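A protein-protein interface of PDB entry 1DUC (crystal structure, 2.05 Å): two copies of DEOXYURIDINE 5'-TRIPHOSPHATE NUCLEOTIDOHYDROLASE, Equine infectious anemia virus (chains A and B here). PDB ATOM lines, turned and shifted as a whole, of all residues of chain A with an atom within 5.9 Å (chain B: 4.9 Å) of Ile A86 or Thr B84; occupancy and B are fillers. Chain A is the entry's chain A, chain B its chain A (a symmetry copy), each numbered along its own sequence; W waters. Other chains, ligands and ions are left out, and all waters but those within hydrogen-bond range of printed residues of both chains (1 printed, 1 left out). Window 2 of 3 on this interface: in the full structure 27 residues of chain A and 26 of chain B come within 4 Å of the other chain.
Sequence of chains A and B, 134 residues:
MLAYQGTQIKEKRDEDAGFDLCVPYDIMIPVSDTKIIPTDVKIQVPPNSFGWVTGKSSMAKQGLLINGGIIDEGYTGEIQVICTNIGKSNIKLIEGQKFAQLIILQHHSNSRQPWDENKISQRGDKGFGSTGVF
ND2 of Asn B67 touches CB of Ala A60, 3.7 Å away. Ala A60 touches Ile B82 (O to CG2, 3.9 Å). CD1 of Leu A65 touches CD2 of Leu B65, 3.9 Å away. Asn B67 touches Leu A65. CD2 of Leu B65 touches CD1 of Ile A86 (3.5 Å). Thr B84 touches Ile A86. CG of Lys A88 touches O of Ser B32, at 3.4 Å.
ND2 of Asn B67 sits at hydrogen-bond distance from O of Leu A64.
Leu A65 touches its own counterpart, Leu B65. Ile A86 touches Leu B65, but with the chains exchanged Leu A65 does not touch Ile B86 (6.6 Å). Ile A86 touches Thr B84, but with the chains exchanged Thr A84 does not touch Ile B86 (8.2 Å). Positions printed for both chains: 32, 63, 64, 65, 84, 85 and 86. Of the 8 pairs that touch across the chains among the printed residues, 1 has its exchanged pair printed and touching as well.
Water W1 lies within hydrogen-bond range of the side-chain amide nitrogen of Asn B67 (2.7 Å), the backbone carbonyl oxygen of Ala A60 (2.7 Å) and the side-chain hydroxyl of Thr B84 (3.0 Å).
Printed residues of chain B within 4 Å of Lys A88: Ser B32 (3.4 Å). Asp B33 touches none of the printed residues of chain A. Of the printed residues of chain A, Ile B82 touches Ala A60 (3.9 Å). Of the printed residues of chain A, Thr B84 touches Ile A86 (3.7 Å). The nearest residue of chain A that does not touch Thr B84 is Ala A60 (5.3 Å).
O of Gly A63 sits at hydrogen-bond distance from N of Ile A86, at 2.8 Å. The backbone NH (N) of Leu A65 sits at hydrogen-bond distance from the backbone carbonyl oxygen (O) of Thr A84 (2.8 Å). O of Asn B85 is in hydrogen-bond range of N of Ser B32. OG1 of Thr B34 lies within hydrogen-bond range of OG1 of Thr B84, at 2.7 Å. O of Thr B84 lies within hydrogen-bond range of N of Leu B65 (2.8 Å). O of Ile B82 lies within hydrogen-bond range of N of Asn B67 (3.0 Å).
Of the 12 printed residues of chain B, 5 touch a printed residue of chain A. Hydrophobic or aromatic side chains of chain B that line the printed part of chain A: Leu B65 and Ile B82. Of the 11 printed residues of chain A, 5 touch a printed residue of chain B. Printed residues of chain A that touch a printed residue of chain B: Ala A60, Leu A64, Leu A65, Ile A86 and Lys A88. Hydrophobic or aromatic side chains of chain A within 4 Å of the printed part of chain B: Ala A60, Leu A65 and Ile A86. Among the printed residues, 8 pairs touch across the chains. Among the printed residues, no Asp or Glu carboxylate lies within 4 Å of a Lys or Arg side-chain nitrogen of the other chain.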
ATOM      1  N   SER A  32     -32.008  15.806 -24.160  1.00  0.00           N
ATOM      2  CA  SER A  32     -32.290  15.095 -22.949  1.00  0.00           C
ATOM      3  C   SER A  32     -32.894  13.734 -23.098  1.00  0.00           C
ATOM      4  O   SER A  32     -33.177  13.140 -22.045  1.00  0.00           O
ATOM      5  CB  SER A  32     -33.302  15.876 -22.047  1.00  0.00           C
ATOM      6  OG  SER A  32     -32.662  17.075 -21.666  1.00  0.00           O
ATOM      7  N   ALA A  60     -19.205  12.989 -29.568  1.00  0.00           N
ATOM      8  CA  ALA A  60     -19.082  13.607 -28.266  1.00  0.00           C
ATOM      9  C   ALA A  60     -19.121  15.120 -28.424  1.00  0.00           C
ATOM     10  O   ALA A  60     -19.736  15.837 -27.595  1.00  0.00           O
ATOM     11  CB  ALA A  60     -17.741  13.241 -27.537  1.00  0.00           C
ATOM     12  N   GLY A  63     -22.524  16.402 -28.214  1.00  0.00           N
ATOM     13  CA  GLY A  63     -23.406  16.178 -27.067  1.00  0.00           C
ATOM     14  C   GLY A  63     -23.963  14.753 -26.986  1.00  0.00           C
ATOM     15  O   GLY A  63     -24.874  14.575 -26.180  1.00  0.00           O
ATOM     16  N   LEU A  64     -23.493  13.804 -27.800  1.00  0.00           N
ATOM     17  CA  LEU A  64     -23.976  12.430 -27.628  1.00  0.00           C
ATOM     18  C   LEU A  64     -23.134  11.802 -26.498  1.00  0.00           C
ATOM     19  O   LEU A  64     -21.899  11.904 -26.530  1.00  0.00           O
ATOM     20  CB  LEU A  64     -23.769  11.593 -28.889  1.00  0.00           C
ATOM     21  CG  LEU A  64     -24.254  10.133 -28.796  1.00  0.00           C
ATOM     22  CD1 LEU A  64     -25.765  10.107 -28.648  1.00  0.00           C
ATOM     23  CD2 LEU A  64     -23.864   9.286 -30.016  1.00  0.00           C
ATOM     24  N   LEU A  65     -23.822  11.207 -25.519  1.00  0.00           N
ATOM     25  CA  LEU A  65     -23.071  10.519 -24.471  1.00  0.00           C
ATOM     26  C   LEU A  65     -23.340   9.025 -24.495  1.00  0.00           C
ATOM     27  O   LEU A  65     -24.533   8.637 -24.547  1.00  0.00           O
ATOM     28  CB  LEU A  65     -23.525  11.108 -23.119  1.00  0.00           C
ATOM     29  CG  LEU A  65     -22.845  10.290 -21.973  1.00  0.00           C
ATOM     30  CD1 LEU A  65     -21.354  10.604 -21.799  1.00  0.00           C
ATOM     31  CD2 LEU A  65     -23.533  10.487 -20.680  1.00  0.00           C
ATOM     32  N   THR A  84     -27.453   9.002 -24.600  1.00  0.00           N
ATOM     33  CA  THR A  84     -28.228  10.105 -24.062  1.00  0.00           C
ATOM     34  C   THR A  84     -27.723  11.369 -24.717  1.00  0.00           C
ATOM     35  O   THR A  84     -26.524  11.571 -24.931  1.00  0.00           O
ATOM     36  CB  THR A  84     -28.089  10.217 -22.518  1.00  0.00           C
ATOM     37  OG1 THR A  84     -28.638   9.023 -21.944  1.00  0.00           O
ATOM     38  CG2 THR A  84     -28.854  11.427 -22.001  1.00  0.00           C
ATOM     39  N   ASN A  85     -28.670  12.242 -25.067  1.00  0.00           N
ATOM     40  CA  ASN A  85     -28.220  13.513 -25.679  1.00  0.00           C
ATOM     41  C   ASN A  85     -28.090  14.507 -24.529  1.00  0.00           C
ATOM     42  O   ASN A  85     -29.131  14.898 -23.945  1.00  0.00           O
ATOM     43  CB  ASN A  85     -29.398  13.910 -26.607  1.00  0.00           C
ATOM     44  CG  ASN A  85     -29.162  15.218 -27.321  1.00  0.00           C
ATOM     45  OD1 ASN A  85     -28.287  16.001 -26.956  1.00  0.00           O
ATOM     46  ND2 ASN A  85     -29.900  15.541 -28.376  1.00  0.00           N
ATOM     47  N   ILE A  86     -26.894  15.006 -24.260  1.00  0.00           N
ATOM     48  CA  ILE A  86     -26.727  15.959 -23.137  1.00  0.00           C
ATOM     49  C   ILE A  86     -26.406  17.302 -23.794  1.00  0.00           C
ATOM     50  O   ILE A  86     -25.875  18.190 -23.157  1.00  0.00           O
ATOM     51  CB  ILE A  86     -25.576  15.501 -22.217  1.00  0.00           C
ATOM     52  CG1 ILE A  86     -24.277  15.236 -23.023  1.00  0.00           C
ATOM     53  CG2 ILE A  86     -25.954  14.189 -21.531  1.00  0.00           C
ATOM     54  CD1 ILE A  86     -23.081  14.913 -22.065  1.00  0.00           C
ATOM     55  N   GLY A  87     -26.590  17.435 -25.082  1.00  0.00           N
ATOM     56  CA  GLY A  87     -26.359  18.699 -25.799  1.00  0.00           C
ATOM     57  C   GLY A  87     -27.623  19.575 -25.794  1.00  0.00           C
ATOM     58  O   GLY A  87     -28.611  19.353 -25.099  1.00  0.00           O
ATOM     59  N   LYS A  88     -27.598  20.594 -26.642  1.00  0.00           N
ATOM     60  CA  LYS A  88     -28.699  21.593 -26.582  1.00  0.00           C
ATOM     61  C   LYS A  88     -29.490  21.480 -27.879  1.00  0.00           C
ATOM     62  O   LYS A  88     -30.402  22.240 -28.157  1.00  0.00           O
ATOM     63  CB  LYS A  88     -28.097  22.992 -26.485  1.00  0.00           C
ATOM     64  CG  LYS A  88     -27.641  23.503 -25.143  1.00  0.00           C
ATOM     65  CD  LYS A  88     -27.186  24.963 -25.247  1.00  0.00           C
ATOM     66  CE  LYS A  88     -27.555  25.709 -23.966  1.00  0.00           C
ATOM     67  N   ILE A  91     -30.239  15.396 -32.007  1.00  0.00           N
ATOM     68  CA  ILE A  91     -29.110  14.744 -32.755  1.00  0.00           C
ATOM     69  C   ILE A  91     -29.740  13.742 -33.726  1.00  0.00           C
ATOM     70  O   ILE A  91     -30.531  12.904 -33.274  1.00  0.00           O
ATOM     71  CB  ILE A  91     -28.213  13.990 -31.757  1.00  0.00           C
ATOM     72  CG1 ILE A  91     -27.425  15.048 -30.955  1.00  0.00           C
ATOM     73  CG2 ILE A  91     -27.275  13.066 -32.578  1.00  0.00           C
ATOM     74  CD1 ILE A  91     -26.761  14.466 -29.688  1.00  0.00           C
ATOM     75  N   SER B  32     -25.756  23.129 -19.453  1.00  0.00           N
ATOM     76  CA  SER B  32     -26.000  22.434 -20.682  1.00  0.00           C
ATOM     77  C   SER B  32     -25.117  22.788 -21.837  1.00  0.00           C
ATOM     78  O   SER B  32     -25.360  22.215 -22.911  1.00  0.00           O
ATOM     79  CB  SER B  32     -27.452  22.686 -21.207  1.00  0.00           C
ATOM     80  OG  SER B  32     -28.330  22.127 -20.252  1.00  0.00           O
ATOM     81  N   ASP B  33     -24.138  23.649 -21.750  1.00  0.00           N
ATOM     82  CA  ASP B  33     -23.350  23.846 -22.989  1.00  0.00           C
ATOM     83  C   ASP B  33     -22.197  22.854 -23.040  1.00  0.00           C
ATOM     84  O   ASP B  33     -21.814  22.323 -21.991  1.00  0.00           O
ATOM     85  CB  ASP B  33     -22.692  25.208 -22.781  1.00  0.00           C
ATOM     86  CG  ASP B  33     -22.529  25.944 -24.101  1.00  0.00           C
ATOM     87  OD1 ASP B  33     -22.855  25.361 -25.168  1.00  0.00           O
ATOM     88  OD2 ASP B  33     -22.060  27.099 -23.967  1.00  0.00           O
ATOM     89  N   THR B  34     -21.582  22.782 -24.191  1.00  0.00           N
ATOM     90  CA  THR B  34     -20.439  21.958 -24.448  1.00  0.00           C
ATOM     91  C   THR B  34     -19.318  22.857 -24.977  1.00  0.00           C
ATOM     92  O   THR B  34     -19.632  23.638 -25.891  1.00  0.00           O
ATOM     93  CB  THR B  34     -20.801  20.875 -25.465  1.00  0.00           C
ATOM     94  OG1 THR B  34     -21.722  19.954 -24.876  1.00  0.00           O
ATOM     95  CG2 THR B  34     -19.515  20.089 -25.844  1.00  0.00           C
ATOM     96  N   GLY B  63     -20.517  18.935 -11.599  1.00  0.00           N
ATOM     97  CA  GLY B  63     -21.306  18.790 -12.823  1.00  0.00           C
ATOM     98  C   GLY B  63     -20.487  18.950 -14.107  1.00  0.00           C
ATOM     99  O   GLY B  63     -21.131  19.059 -15.149  1.00  0.00           O
ATOM    100  N   LEU B  64     -19.154  19.013 -14.047  1.00  0.00           N
ATOM    101  CA  LEU B  64     -18.396  19.065 -15.301  1.00  0.00           C
ATOM    102  C   LEU B  64     -18.249  17.609 -15.790  1.00  0.00           C
ATOM    103  O   LEU B  64     -17.861  16.737 -15.000  1.00  0.00           O
ATOM    104  CB  LEU B  64     -16.994  19.635 -15.095  1.00  0.00           C
ATOM    105  CG  LEU B  64     -16.128  19.728 -16.367  1.00  0.00           C
ATOM    106  CD1 LEU B  64     -16.738  20.736 -17.325  1.00  0.00           C
ATOM    107  CD2 LEU B  64     -14.674  20.135 -16.083  1.00  0.00           C
ATOM    108  N   LEU B  65     -18.597  17.382 -17.061  1.00  0.00           N
ATOM    109  CA  LEU B  65     -18.393  16.039 -17.600  1.00  0.00           C
ATOM    110  C   LEU B  65     -17.359  16.047 -18.712  1.00  0.00           C
ATOM    111  O   LEU B  65     -17.471  16.905 -19.622  1.00  0.00           O
ATOM    112  CB  LEU B  65     -19.750  15.556 -18.154  1.00  0.00           C
ATOM    113  CG  LEU B  65     -19.528  14.183 -18.868  1.00  0.00           C
ATOM    114  CD1 LEU B  65     -19.320  13.015 -17.895  1.00  0.00           C
ATOM    115  CD2 LEU B  65     -20.643  13.856 -19.781  1.00  0.00           C
ATOM    116  N   ASN B  67     -16.189  14.309 -21.987  1.00  0.00           N
ATOM    117  CA  ASN B  67     -16.767  13.286 -22.843  1.00  0.00           C
ATOM    118  C   ASN B  67     -15.795  12.978 -23.989  1.00  0.00           C
ATOM    119  O   ASN B  67     -14.774  13.666 -24.148  1.00  0.00           O
ATOM    120  CB  ASN B  67     -17.997  13.967 -23.505  1.00  0.00           C
ATOM    121  CG  ASN B  67     -18.934  12.886 -24.056  1.00  0.00           C
ATOM    122  OD1 ASN B  67     -18.627  11.688 -23.939  1.00  0.00           O
ATOM    123  ND2 ASN B  67     -20.018  13.344 -24.664  1.00  0.00           N
ATOM    124  N   ILE B  82     -13.094  17.653 -24.332  1.00  0.00           N
ATOM    125  CA  ILE B  82     -14.468  18.024 -24.679  1.00  0.00           C
ATOM    126  C   ILE B  82     -15.275  18.138 -23.390  1.00  0.00           C
ATOM    127  O   ILE B  82     -15.330  17.086 -22.741  1.00  0.00           O
ATOM    128  CB  ILE B  82     -15.056  16.931 -25.619  1.00  0.00           C
ATOM    129  CG1 ILE B  82     -14.197  16.861 -26.874  1.00  0.00           C
ATOM    130  CG2 ILE B  82     -16.544  17.282 -25.954  1.00  0.00           C
ATOM    131  CD1 ILE B  82     -14.538  15.623 -27.768  1.00  0.00           C
ATOM    132  N   CYS B  83     -15.799  19.280 -22.957  1.00  0.00           N
ATOM    133  CA  CYS B  83     -16.408  19.417 -21.640  1.00  0.00           C
ATOM    134  C   CYS B  83     -17.887  19.785 -21.784  1.00  0.00           C
ATOM    135  O   CYS B  83     -18.149  20.700 -22.581  1.00  0.00           O
ATOM    136  CB  CYS B  83     -15.773  20.695 -20.938  1.00  0.00           C
ATOM    137  SG  CYS B  83     -14.018  20.356 -20.642  1.00  0.00           S
ATOM    138  N   THR B  84     -18.771  19.135 -21.034  1.00  0.00           N
ATOM    139  CA  THR B  84     -20.177  19.499 -21.032  1.00  0.00           C
ATOM    140  C   THR B  84     -20.576  19.738 -19.595  1.00  0.00           C
ATOM    141  O   THR B  84     -20.174  19.027 -18.669  1.00  0.00           O
ATOM    142  CB  THR B  84     -21.069  18.387 -21.651  1.00  0.00           C
ATOM    143  OG1 THR B  84     -20.693  18.245 -23.029  1.00  0.00           O
ATOM    144  CG2 THR B  84     -22.538  18.773 -21.564  1.00  0.00           C
ATOM    145  N   ASN B  85     -21.377  20.787 -19.396  1.00  0.00           N
ATOM    146  CA  ASN B  85     -21.825  21.038 -18.008  1.00  0.00           C
ATOM    147  C   ASN B  85     -23.161  20.316 -17.864  1.00  0.00           C
ATOM    148  O   ASN B  85     -24.155  20.746 -18.499  1.00  0.00           O
ATOM    149  CB  ASN B  85     -22.033  22.575 -17.963  1.00  0.00           C
ATOM    150  CG  ASN B  85     -22.530  23.056 -16.622  1.00  0.00           C
ATOM    151  OD1 ASN B  85     -23.001  22.278 -15.794  1.00  0.00           O
ATOM    152  ND2 ASN B  85     -22.452  24.344 -16.308  1.00  0.00           N
ATOM    153  N   ILE B  86     -23.252  19.327 -16.988  1.00  0.00           N
ATOM    154  CA  ILE B  86     -24.529  18.590 -16.835  1.00  0.00           C
ATOM    155  C   ILE B  86     -25.052  18.977 -15.451  1.00  0.00           C
ATOM    156  O   ILE B  86     -25.879  18.286 -14.889  1.00  0.00           O
ATOM    157  CB  ILE B  86     -24.281  17.071 -16.932  1.00  0.00           C
ATOM    158  CG1 ILE B  86     -23.165  16.615 -15.956  1.00  0.00           C
ATOM    159  CG2 ILE B  86     -23.817  16.711 -18.344  1.00  0.00           C
ATOM    160  CD1 ILE B  86     -23.022  15.055 -15.957  1.00  0.00           C
HETATM  161  O   HOH W   1     -20.319  16.004 -24.947  1.00  0.00           O
